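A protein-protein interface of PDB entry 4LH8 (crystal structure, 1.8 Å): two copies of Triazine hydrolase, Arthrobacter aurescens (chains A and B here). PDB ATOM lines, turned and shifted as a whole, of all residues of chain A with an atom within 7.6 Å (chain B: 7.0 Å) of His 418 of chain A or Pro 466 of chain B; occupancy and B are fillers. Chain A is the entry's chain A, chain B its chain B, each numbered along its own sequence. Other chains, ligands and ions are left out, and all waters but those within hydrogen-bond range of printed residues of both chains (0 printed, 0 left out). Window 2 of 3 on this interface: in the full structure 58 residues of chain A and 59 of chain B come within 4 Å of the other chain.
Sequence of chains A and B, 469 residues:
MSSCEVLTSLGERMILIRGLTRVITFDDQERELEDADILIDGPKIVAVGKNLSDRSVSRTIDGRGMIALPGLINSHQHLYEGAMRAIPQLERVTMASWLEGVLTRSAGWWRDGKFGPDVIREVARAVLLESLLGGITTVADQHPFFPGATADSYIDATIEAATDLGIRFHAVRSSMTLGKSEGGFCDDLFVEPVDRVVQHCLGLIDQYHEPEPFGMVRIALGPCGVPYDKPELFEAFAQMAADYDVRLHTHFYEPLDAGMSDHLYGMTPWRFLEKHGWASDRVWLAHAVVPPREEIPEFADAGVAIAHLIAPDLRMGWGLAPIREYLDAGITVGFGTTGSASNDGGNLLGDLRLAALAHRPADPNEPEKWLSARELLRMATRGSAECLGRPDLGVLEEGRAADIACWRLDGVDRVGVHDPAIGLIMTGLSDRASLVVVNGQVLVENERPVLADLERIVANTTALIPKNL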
ATOM      1  N   ARG A  22     -16.602  -6.272  14.076  1.00  0.00           N
ATOM      2  CA  ARG A  22     -15.887  -5.093  13.602  1.00  0.00           C
ATOM      3  C   ARG A  22     -16.280  -4.802  12.159  1.00  0.00           C
ATOM      4  O   ARG A  22     -16.377  -5.721  11.345  1.00  0.00           O
ATOM      5  CB  ARG A  22     -14.370  -5.302  13.709  1.00  0.00           C
ATOM      6  CG  ARG A  22     -13.511  -4.180  13.117  1.00  0.00           C
ATOM      7  CD  ARG A  22     -13.474  -2.928  14.004  1.00  0.00           C
ATOM      8  NE  ARG A  22     -12.921  -3.209  15.329  1.00  0.00           N
ATOM      9  CZ  ARG A  22     -11.916  -2.546  15.895  1.00  0.00           C
ATOM     10  NH1 ARG A  22     -11.320  -1.536  15.263  1.00  0.00           N
ATOM     11  NH2 ARG A  22     -11.502  -2.898  17.102  1.00  0.00           N
ATOM     12  N   ARG A 414      -6.658 -17.644  15.378  1.00  0.00           N
ATOM     13  CA  ARG A 414      -6.698 -16.197  15.599  1.00  0.00           C
ATOM     14  C   ARG A 414      -6.920 -15.844  17.075  1.00  0.00           C
ATOM     15  O   ARG A 414      -7.224 -14.700  17.408  1.00  0.00           O
ATOM     16  CB  ARG A 414      -7.746 -15.517  14.703  1.00  0.00           C
ATOM     17  CG  ARG A 414      -7.521 -15.717  13.187  1.00  0.00           C
ATOM     18  CD  ARG A 414      -8.445 -14.825  12.370  1.00  0.00           C
ATOM     19  NE  ARG A 414      -8.545 -15.198  10.956  1.00  0.00           N
ATOM     20  CZ  ARG A 414      -7.685 -14.809  10.016  1.00  0.00           C
ATOM     21  NH1 ARG A 414      -6.645 -14.058  10.336  1.00  0.00           N
ATOM     22  NH2 ARG A 414      -7.853 -15.186   8.754  1.00  0.00           N
ATOM     23  N   VAL A 415      -6.761 -16.828  17.957  1.00  0.00           N
ATOM     24  CA  VAL A 415      -6.819 -16.569  19.390  1.00  0.00           C
ATOM     25  C   VAL A 415      -5.698 -15.595  19.769  1.00  0.00           C
ATOM     26  O   VAL A 415      -4.583 -15.692  19.255  1.00  0.00           O
ATOM     27  CB  VAL A 415      -6.702 -17.885  20.198  1.00  0.00           C
ATOM     28  CG1 VAL A 415      -6.303 -17.610  21.643  1.00  0.00           C
ATOM     29  CG2 VAL A 415      -8.008 -18.670  20.129  1.00  0.00           C
ATOM     30  N   GLY A 416      -5.998 -14.637  20.641  1.00  0.00           N
ATOM     31  CA  GLY A 416      -4.985 -13.708  21.117  1.00  0.00           C
ATOM     32  C   GLY A 416      -4.716 -12.524  20.203  1.00  0.00           C
ATOM     33  O   GLY A 416      -3.822 -11.716  20.471  1.00  0.00           O
ATOM     34  N   VAL A 417      -5.479 -12.416  19.119  1.00  0.00           N
ATOM     35  CA  VAL A 417      -5.380 -11.252  18.243  1.00  0.00           C
ATOM     36  C   VAL A 417      -5.971 -10.030  18.932  1.00  0.00           C
ATOM     37  O   VAL A 417      -7.095 -10.074  19.431  1.00  0.00           O
ATOM     38  CB  VAL A 417      -6.109 -11.474  16.909  1.00  0.00           C
ATOM     39  CG1 VAL A 417      -6.397 -10.140  16.226  1.00  0.00           C
ATOM     40  CG2 VAL A 417      -5.291 -12.385  16.002  1.00  0.00           C
ATOM     41  N   HIS A 418      -5.210  -8.940  18.962  1.00  0.00           N
ATOM     42  CA  HIS A 418      -5.646  -7.731  19.651  1.00  0.00           C
ATOM     43  C   HIS A 418      -6.338  -6.721  18.735  1.00  0.00           C
ATOM     44  O   HIS A 418      -7.317  -6.095  19.133  1.00  0.00           O
ATOM     45  CB  HIS A 418      -4.483  -7.108  20.426  1.00  0.00           C
ATOM     46  CG  HIS A 418      -4.008  -7.962  21.558  1.00  0.00           C
ATOM     47  ND1 HIS A 418      -4.544  -7.880  22.826  1.00  0.00           N
ATOM     48  CD2 HIS A 418      -3.073  -8.941  21.606  1.00  0.00           C
ATOM     49  CE1 HIS A 418      -3.949  -8.762  23.610  1.00  0.00           C
ATOM     50  NE2 HIS A 418      -3.054  -9.419  22.894  1.00  0.00           N
ATOM     51  N   ASP A 419      -5.848  -6.582  17.505  1.00  0.00           N
ATOM     52  CA  ASP A 419      -6.473  -5.700  16.522  1.00  0.00           C
ATOM     53  C   ASP A 419      -6.881  -6.560  15.327  1.00  0.00           C
ATOM     54  O   ASP A 419      -6.030  -7.155  14.680  1.00  0.00           O
ATOM     55  CB  ASP A 419      -5.484  -4.600  16.104  1.00  0.00           C
ATOM     56  CG  ASP A 419      -6.024  -3.692  15.003  1.00  0.00           C
ATOM     57  OD1 ASP A 419      -6.738  -4.163  14.096  1.00  0.00           O
ATOM     58  OD2 ASP A 419      -5.711  -2.488  15.031  1.00  0.00           O
ATOM     59  N   PRO A 420      -8.190  -6.640  15.042  1.00  0.00           N
ATOM     60  CA  PRO A 420      -8.686  -7.588  14.032  1.00  0.00           C
ATOM     61  C   PRO A 420      -8.313  -7.229  12.598  1.00  0.00           C
ATOM     62  O   PRO A 420      -8.182  -8.136  11.775  1.00  0.00           O
ATOM     63  CB  PRO A 420     -10.209  -7.522  14.207  1.00  0.00           C
ATOM     64  CG  PRO A 420     -10.457  -6.156  14.757  1.00  0.00           C
ATOM     65  CD  PRO A 420      -9.285  -5.864  15.654  1.00  0.00           C
ATOM     66  N   ALA A 421      -8.158  -5.948  12.287  1.00  0.00           N
ATOM     67  CA  ALA A 421      -7.709  -5.573  10.951  1.00  0.00           C
ATOM     68  C   ALA A 421      -6.273  -6.048  10.704  1.00  0.00           C
ATOM     69  O   ALA A 421      -5.972  -6.619   9.657  1.00  0.00           O
ATOM     70  CB  ALA A 421      -7.836  -4.064  10.735  1.00  0.00           C
ATOM     71  N   ILE A 422      -5.393  -5.811  11.673  1.00  0.00           N
ATOM     72  CA  ILE A 422      -4.019  -6.304  11.599  1.00  0.00           C
ATOM     73  C   ILE A 422      -4.052  -7.834  11.607  1.00  0.00           C
ATOM     74  O   ILE A 422      -3.315  -8.501  10.879  1.00  0.00           O
ATOM     75  CB  ILE A 422      -3.178  -5.793  12.790  1.00  0.00           C
ATOM     76  CG1 ILE A 422      -3.048  -4.263  12.734  1.00  0.00           C
ATOM     77  CG2 ILE A 422      -1.805  -6.455  12.805  1.00  0.00           C
ATOM     78  CD1 ILE A 422      -2.278  -3.658  13.905  1.00  0.00           C
ATOM     79  N   GLY A 423      -4.934  -8.384  12.429  1.00  0.00           N
ATOM     80  CA  GLY A 423      -5.064  -9.822  12.539  1.00  0.00           C
ATOM     81  C   GLY A 423      -5.396 -10.463  11.205  1.00  0.00           C
ATOM     82  O   GLY A 423      -4.899 -11.535  10.884  1.00  0.00           O
ATOM     83  N   THR A 427      -2.167 -13.004  10.747  1.00  0.00           N
ATOM     84  CA  THR A 427      -2.388 -14.296  11.382  1.00  0.00           C
ATOM     85  C   THR A 427      -3.201 -15.195  10.469  1.00  0.00           C
ATOM     86  O   THR A 427      -3.755 -14.738   9.473  1.00  0.00           O
ATOM     87  CB  THR A 427      -3.161 -14.153  12.708  1.00  0.00           C
ATOM     88  OG1 THR A 427      -4.488 -13.671  12.442  1.00  0.00           O
ATOM     89  CG2 THR A 427      -2.443 -13.178  13.643  1.00  0.00           C
ATOM     90  N   GLY B  82       1.623 -16.211  21.854  1.00  0.00           N
ATOM     91  CA  GLY B  82       0.329 -16.364  21.219  1.00  0.00           C
ATOM     92  C   GLY B  82      -0.640 -15.315  21.737  1.00  0.00           C
ATOM     93  O   GLY B  82      -1.576 -14.922  21.046  1.00  0.00           O
ATOM     94  N   ALA B  83      -0.407 -14.852  22.961  1.00  0.00           N
ATOM     95  CA  ALA B  83      -1.286 -13.859  23.577  1.00  0.00           C
ATOM     96  C   ALA B  83      -0.884 -12.429  23.217  1.00  0.00           C
ATOM     97  O   ALA B  83      -1.426 -11.471  23.771  1.00  0.00           O
ATOM     98  CB  ALA B  83      -1.290 -14.036  25.100  1.00  0.00           C
ATOM     99  N   MET B  84       0.069 -12.286  22.299  1.00  0.00           N
ATOM    100  CA  MET B  84       0.603 -10.967  21.952  1.00  0.00           C
ATOM    101  C   MET B  84       0.499 -10.680  20.455  1.00  0.00           C
ATOM    102  O   MET B  84       1.360 -10.009  19.889  1.00  0.00           O
ATOM    103  CB  MET B  84       2.067 -10.849  22.393  1.00  0.00           C
ATOM    104  CG  MET B  84       2.309 -11.123  23.874  1.00  0.00           C
ATOM    105  SD  MET B  84       4.060 -11.029  24.321  1.00  0.00           S
ATOM    106  CE  MET B  84       4.375  -9.300  24.016  1.00  0.00           C
ATOM    107  N   ARG B  85      -0.549 -11.197  19.820  1.00  0.00           N
ATOM    108  CA  ARG B  85      -0.727 -11.040  18.376  1.00  0.00           C
ATOM    109  C   ARG B  85      -1.398  -9.722  17.973  1.00  0.00           C
ATOM    110  O   ARG B  85      -2.296  -9.233  18.658  1.00  0.00           O
ATOM    111  CB  ARG B  85      -1.556 -12.202  17.823  1.00  0.00           C
ATOM    112  CG  ARG B  85      -0.820 -13.521  17.771  1.00  0.00           C
ATOM    113  CD  ARG B  85      -1.801 -14.648  17.446  1.00  0.00           C
ATOM    114  NE  ARG B  85      -1.080 -15.832  17.012  1.00  0.00           N
ATOM    115  CZ  ARG B  85      -1.565 -17.067  17.043  1.00  0.00           C
ATOM    116  NH1 ARG B  85      -2.791 -17.287  17.492  1.00  0.00           N
ATOM    117  NH2 ARG B  85      -0.809 -18.080  16.625  1.00  0.00           N
ATOM    118  N   ALA B  86      -0.965  -9.167  16.844  1.00  0.00           N
ATOM    119  CA  ALA B  86      -1.635  -8.016  16.242  1.00  0.00           C
ATOM    120  C   ALA B  86      -1.861  -6.884  17.247  1.00  0.00           C
ATOM    121  O   ALA B  86      -2.937  -6.283  17.302  1.00  0.00           O
ATOM    122  CB  ALA B  86      -2.953  -8.446  15.606  1.00  0.00           C
ATOM    123  N   ILE B  87      -0.848  -6.615  18.061  1.00  0.00           N
ATOM    124  CA  ILE B  87      -0.882  -5.462  18.948  1.00  0.00           C
ATOM    125  C   ILE B  87      -0.441  -4.238  18.154  1.00  0.00           C
ATOM    126  O   ILE B  87       0.684  -4.201  17.648  1.00  0.00           O
ATOM    127  CB  ILE B  87       0.046  -5.652  20.155  1.00  0.00           C
ATOM    128  CG1 ILE B  87      -0.474  -6.790  21.043  1.00  0.00           C
ATOM    129  CG2 ILE B  87       0.154  -4.343  20.936  1.00  0.00           C
ATOM    130  CD1 ILE B  87       0.460  -7.167  22.169  1.00  0.00           C
ATOM    131  N   PRO B  88      -1.329  -3.240  18.030  1.00  0.00           N
ATOM    132  CA  PRO B  88      -1.081  -2.052  17.196  1.00  0.00           C
ATOM    133  C   PRO B  88       0.249  -1.340  17.473  1.00  0.00           C
ATOM    134  O   PRO B  88       0.922  -0.942  16.521  1.00  0.00           O
ATOM    135  CB  PRO B  88      -2.260  -1.132  17.532  1.00  0.00           C
ATOM    136  CG  PRO B  88      -3.358  -2.067  17.939  1.00  0.00           C
ATOM    137  CD  PRO B  88      -2.672  -3.216  18.642  1.00  0.00           C
ATOM    138  N   ARG B 105       5.658  -6.510  28.561  1.00  0.00           N
ATOM    139  CA  ARG B 105       4.351  -7.147  28.677  1.00  0.00           C
ATOM    140  C   ARG B 105       4.427  -8.472  29.421  1.00  0.00           C
ATOM    141  O   ARG B 105       3.608  -8.738  30.297  1.00  0.00           O
ATOM    142  CB  ARG B 105       3.705  -7.338  27.298  1.00  0.00           C
ATOM    143  CG  ARG B 105       3.170  -6.051  26.689  1.00  0.00           C
ATOM    144  CD  ARG B 105       2.582  -6.283  25.294  1.00  0.00           C
ATOM    145  NE  ARG B 105       1.977  -5.069  24.746  1.00  0.00           N
ATOM    146  CZ  ARG B 105       2.670  -4.000  24.362  1.00  0.00           C
ATOM    147  NH1 ARG B 105       2.046  -2.928  23.878  1.00  0.00           N
ATOM    148  NH2 ARG B 105       3.992  -3.999  24.468  1.00  0.00           N
ATOM    149  N   TRP B 109       2.414  -8.399  32.848  1.00  0.00           N
ATOM    150  CA  TRP B 109       1.273  -9.296  32.984  1.00  0.00           C
ATOM    151  C   TRP B 109       1.541 -10.299  34.094  1.00  0.00           C
ATOM    152  O   TRP B 109       0.659 -10.603  34.894  1.00  0.00           O
ATOM    153  CB  TRP B 109       1.006 -10.050  31.677  1.00  0.00           C
ATOM    154  CG  TRP B 109       0.474  -9.202  30.562  1.00  0.00           C
ATOM    155  CD1 TRP B 109      -0.060  -7.948  30.663  1.00  0.00           C
ATOM    156  CD2 TRP B 109       0.433  -9.546  29.170  1.00  0.00           C
ATOM    157  NE1 TRP B 109      -0.430  -7.490  29.420  1.00  0.00           N
ATOM    158  CE2 TRP B 109      -0.140  -8.452  28.487  1.00  0.00           C
ATOM    159  CE3 TRP B 109       0.825 -10.670  28.437  1.00  0.00           C
ATOM    160  CZ2 TRP B 109      -0.332  -8.454  27.106  1.00  0.00           C
ATOM    161  CZ3 TRP B 109       0.633 -10.668  27.066  1.00  0.00           C
ATOM    162  CH2 TRP B 109       0.064  -9.568  26.416  1.00  0.00           C
ATOM    163  N   LYS B 114      -1.642 -12.065  35.631  1.00  0.00           N
ATOM    164  CA  LYS B 114      -2.397 -12.243  34.393  1.00  0.00           C
ATOM    165  C   LYS B 114      -1.742 -13.284  33.493  1.00  0.00           C
ATOM    166  O   LYS B 114      -2.277 -13.629  32.432  1.00  0.00           O
ATOM    167  CB  LYS B 114      -2.477 -10.921  33.625  1.00  0.00           C
ATOM    168  CG  LYS B 114      -3.326  -9.830  34.260  1.00  0.00           C
ATOM    169  CD  LYS B 114      -3.072  -8.515  33.535  1.00  0.00           C
ATOM    170  CE  LYS B 114      -4.071  -7.434  33.898  1.00  0.00           C
ATOM    171  NZ  LYS B 114      -5.456  -7.786  33.487  1.00  0.00           N
ATOM    172  N   PHE B 115      -0.584 -13.779  33.921  1.00  0.00           N
ATOM    173  CA  PHE B 115       0.242 -14.647  33.092  1.00  0.00           C
ATOM    174  C   PHE B 115       0.709 -15.867  33.874  1.00  0.00           C
ATOM    175  O   PHE B 115       1.862 -16.279  33.763  1.00  0.00           O
ATOM    176  CB  PHE B 115       1.458 -13.876  32.576  1.00  0.00           C
ATOM    177  CG  PHE B 115       1.660 -13.980  31.089  1.00  0.00           C
ATOM    178  CD1 PHE B 115       0.596 -14.271  30.244  1.00  0.00           C
ATOM    179  CD2 PHE B 115       2.916 -13.789  30.536  1.00  0.00           C
ATOM    180  CE1 PHE B 115       0.780 -14.365  28.871  1.00  0.00           C
ATOM    181  CE2 PHE B 115       3.110 -13.886  29.163  1.00  0.00           C
ATOM    182  CZ  PHE B 115       2.040 -14.173  28.331  1.00  0.00           C
ATOM    183  N   VAL B 119      -2.240 -19.829  32.462  1.00  0.00           N
ATOM    184  CA  VAL B 119      -2.532 -18.999  31.298  1.00  0.00           C
ATOM    185  C   VAL B 119      -1.659 -19.469  30.137  1.00  0.00           C
ATOM    186  O   VAL B 119      -2.132 -19.613  29.013  1.00  0.00           O
ATOM    187  CB  VAL B 119      -2.287 -17.497  31.564  1.00  0.00           C
ATOM    188  CG1 VAL B 119      -2.456 -16.683  30.274  1.00  0.00           C
ATOM    189  CG2 VAL B 119      -3.233 -16.988  32.640  1.00  0.00           C
ATOM    190  N   VAL B 123      -2.655 -20.956  26.370  1.00  0.00           N
ATOM    191  CA  VAL B 123      -2.134 -20.272  25.196  1.00  0.00           C
ATOM    192  C   VAL B 123      -1.358 -21.286  24.370  1.00  0.00           C
ATOM    193  O   VAL B 123      -1.534 -21.363  23.162  1.00  0.00           O
ATOM    194  CB  VAL B 123      -1.234 -19.083  25.558  1.00  0.00           C
ATOM    195  CG1 VAL B 123      -0.527 -18.570  24.322  1.00  0.00           C
ATOM    196  CG2 VAL B 123      -2.058 -17.971  26.209  1.00  0.00           C
ATOM    197  N   THR B 461      -9.234 -20.526  26.097  1.00  0.00           N
ATOM    198  CA  THR B 461      -8.014 -19.752  25.944  1.00  0.00           C
ATOM    199  C   THR B 461      -8.302 -18.267  25.786  1.00  0.00           C
ATOM    200  O   THR B 461      -7.591 -17.427  26.338  1.00  0.00           O
ATOM    201  CB  THR B 461      -7.193 -20.238  24.746  1.00  0.00           C
ATOM    202  OG1 THR B 461      -6.892 -21.630  24.915  1.00  0.00           O
ATOM    203  CG2 THR B 461      -5.897 -19.445  24.637  1.00  0.00           C
ATOM    204  N   THR B 462      -9.338 -17.952  25.014  1.00  0.00           N
ATOM    205  CA  THR B 462      -9.709 -16.570  24.748  1.00  0.00           C
ATOM    206  C   THR B 462     -10.043 -15.853  26.050  1.00  0.00           C
ATOM    207  O   THR B 462      -9.699 -14.690  26.235  1.00  0.00           O
ATOM    208  CB  THR B 462     -10.921 -16.487  23.796  1.00  0.00           C
ATOM    209  OG1 THR B 462     -10.564 -17.018  22.512  1.00  0.00           O
ATOM    210  CG2 THR B 462     -11.382 -15.040  23.638  1.00  0.00           C
ATOM    211  N   ALA B 463     -10.705 -16.563  26.954  1.00  0.00           N
ATOM    212  CA  ALA B 463     -11.080 -15.992  28.243  1.00  0.00           C
ATOM    213  C   ALA B 463      -9.863 -15.609  29.087  1.00  0.00           C
ATOM    214  O   ALA B 463      -9.963 -14.774  29.994  1.00  0.00           O
ATOM    215  CB  ALA B 463     -11.965 -16.962  29.000  1.00  0.00           C
ATOM    216  N   LEU B 464      -8.717 -16.209  28.774  1.00  0.00           N
ATOM    217  CA  LEU B 464      -7.503 -16.064  29.582  1.00  0.00           C
ATOM    218  C   LEU B 464      -6.462 -15.104  28.993  1.00  0.00           C
ATOM    219  O   LEU B 464      -5.475 -14.774  29.649  1.00  0.00           O
ATOM    220  CB  LEU B 464      -6.862 -17.437  29.819  1.00  0.00           C
ATOM    221  CG  LEU B 464      -7.677 -18.451  30.628  1.00  0.00           C
ATOM    222  CD1 LEU B 464      -7.133 -19.855  30.446  1.00  0.00           C
ATOM    223  CD2 LEU B 464      -7.711 -18.080  32.101  1.00  0.00           C
ATOM    224  N   ILE B 465      -6.668 -14.664  27.758  1.00  0.00           N
ATOM    225  CA  ILE B 465      -5.744 -13.721  27.144  1.00  0.00           C
ATOM    226  C   ILE B 465      -5.807 -12.430  27.954  1.00  0.00           C
ATOM    227  O   ILE B 465      -6.892 -11.890  28.159  1.00  0.00           O
ATOM    228  CB  ILE B 465      -6.147 -13.425  25.689  1.00  0.00           C
ATOM    229  CG1 ILE B 465      -6.175 -14.717  24.875  1.00  0.00           C
ATOM    230  CG2 ILE B 465      -5.181 -12.431  25.053  1.00  0.00           C
ATOM    231  CD1 ILE B 465      -4.819 -15.377  24.760  1.00  0.00           C
ATOM    232  N   PRO B 466      -4.653 -11.944  28.441  1.00  0.00           N
ATOM    233  CA  PRO B 466      -4.640 -10.689  29.204  1.00  0.00           C
ATOM    234  C   PRO B 466      -5.337  -9.574  28.433  1.00  0.00           C
ATOM    235  O   PRO B 466      -4.936  -9.257  27.310  1.00  0.00           O
ATOM    236  CB  PRO B 466      -3.146 -10.387  29.350  1.00  0.00           C
ATOM    237  CG  PRO B 466      -2.501 -11.731  29.327  1.00  0.00           C
ATOM    238  CD  PRO B 466      -3.309 -12.543  28.344  1.00  0.00           C
ATOM    239  N   LYS B 467      -6.376  -8.999  29.033  1.00  0.00           N
ATOM    240  CA  LYS B 467      -7.190  -7.989  28.367  1.00  0.00           C
ATOM    241  C   LYS B 467      -6.514  -6.623  28.396  1.00  0.00           C
ATOM    242  O   LYS B 467      -6.102  -6.153  29.455  1.00  0.00           O
ATOM    243  CB  LYS B 467      -8.573  -7.903  29.017  1.00  0.00           C
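No position is printed for both chains.
Of the 18 pairs that touch across the chains among the printed residues, none has its exchanged pair printed and touching as well.
His 418 of chain A touches just these residues of chain B: Ala 83, Arg 85, Ala 86, Ile 87 and Pro 466.
Printed residues of chain B within 4 Å of Asp 419 of chain A: Ala 86 and Pro 88.
Thr 427 of chain A touches none of the printed residues of chain B.
Of the printed residues of chain A, Gly 82 of chain B touches Val 415 (3.6 Å) and Gly 416 (3.6 Å).
Of the printed residues of chain A, Ile 87 of chain B touches His 418 (3.4 Å).
Of the printed residues of chain A, Thr 461 of chain B touches Val 415 (3.5 Å).
Of chain A, only His 418 (3.9 Å) comes within 4 Å of Pro 466 of chain B.
The nearest residue of chain A that does not touch Pro 466 of chain B is Gly 416 of chain A (7.4 Å).
The nearest printed residue of chain A that does not touch Ala 86 of chain B is Thr 427 of chain A (5.1 Å).
Printed residues of chain B that touch a printed residue of chain A: Gly 82, Ala 83, Arg 85, Ala 86, Ile 87, Pro 88, Thr 461, Thr 462 and Pro 466.
Along chain B the printed residues that touch a printed residue of chain A span positions 82 to 466.
Of the 12 printed residues of chain A, 7 touch a printed residue of chain B.
Printed residues of chain A that touch a printed residue of chain B: Val 415, Gly 416, Val 417, His 418, Asp 419, Ile 422 and Gly 423.
Hydrophobic or aromatic side chains of chain A within 4 Å of the printed part of chain B: Val 415, Val 417, His 418 and Ile 422.
Among the printed residues, 18 pairs touch across the chains.
The backbone NH (N) of Arg 85 of chain B sits at hydrogen-bond distance from the backbone carbonyl oxygen (O) of Gly 416 of chain A (3.4 Å).
N of Asp 419 of chain A lies within hydrogen-bond range of O of Ala 86 of chain B (2.9 Å).
O of Val 415 of chain A sits at hydrogen-bond distance from NH1 of Arg 85 of chain B (3.0 Å).
NE2 of His 418 of chain A sits at hydrogen-bond distance from O of Ala 83 of chain B (2.8 Å).
N of His 418 of chain A lies within hydrogen-bond range of O of Arg 85 of chain B.
The side-chain carboxylate (OD1) of Asp 419 of chain A is in hydrogen-bond range of the backbone NH (N) of Ile 422 of chain A (3.2 Å).
The backbone carbonyl oxygen (O) of Gly 416 of chain A sits close to a ring nitrogen (NE2) of His 418 of chain A (3.4 Å).
The backbone NH of Ala 421 of chain A sits at hydrogen-bond distance from the side-chain carboxylate of Asp 419 of chain A (2.9 Å).
The side-chain hydroxyl of Thr 427 of chain A lies within hydrogen-bond range of the backbone carbonyl oxygen of Gly 423 of chain A (2.7 Å).
The guanidinium group of Arg 414 of chain A sits at hydrogen-bond distance from the backbone carbonyl oxygen of Gly 423 of chain A, at 3.1 Å.
Among the printed residues, merely in contact across the chains: Val 415 of chain A with Gly 82 of chain B, Val 415 of chain A with Thr 461 of chain B, Val 415 of chain A with Thr 462 of chain B, Gly 416 of chain A with Gly 82 of chain B, Val 417 of chain A with Arg 85 of chain B, Val 417 of chain A with Ala 86 of chain B, His 418 of chain A with Ala 86 of chain B, His 418 of chain A with Ile 87 of chain B, His 418 of chain A with Pro 466 of chain B, Asp 419 of chain A with Pro 88 of chain B, Ile 422 of chain A with Ala 86 of chain B, Ile 422 of chain A with Pro 88 of chain B and Gly 423 of chain A with Ala 86 of chain B.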
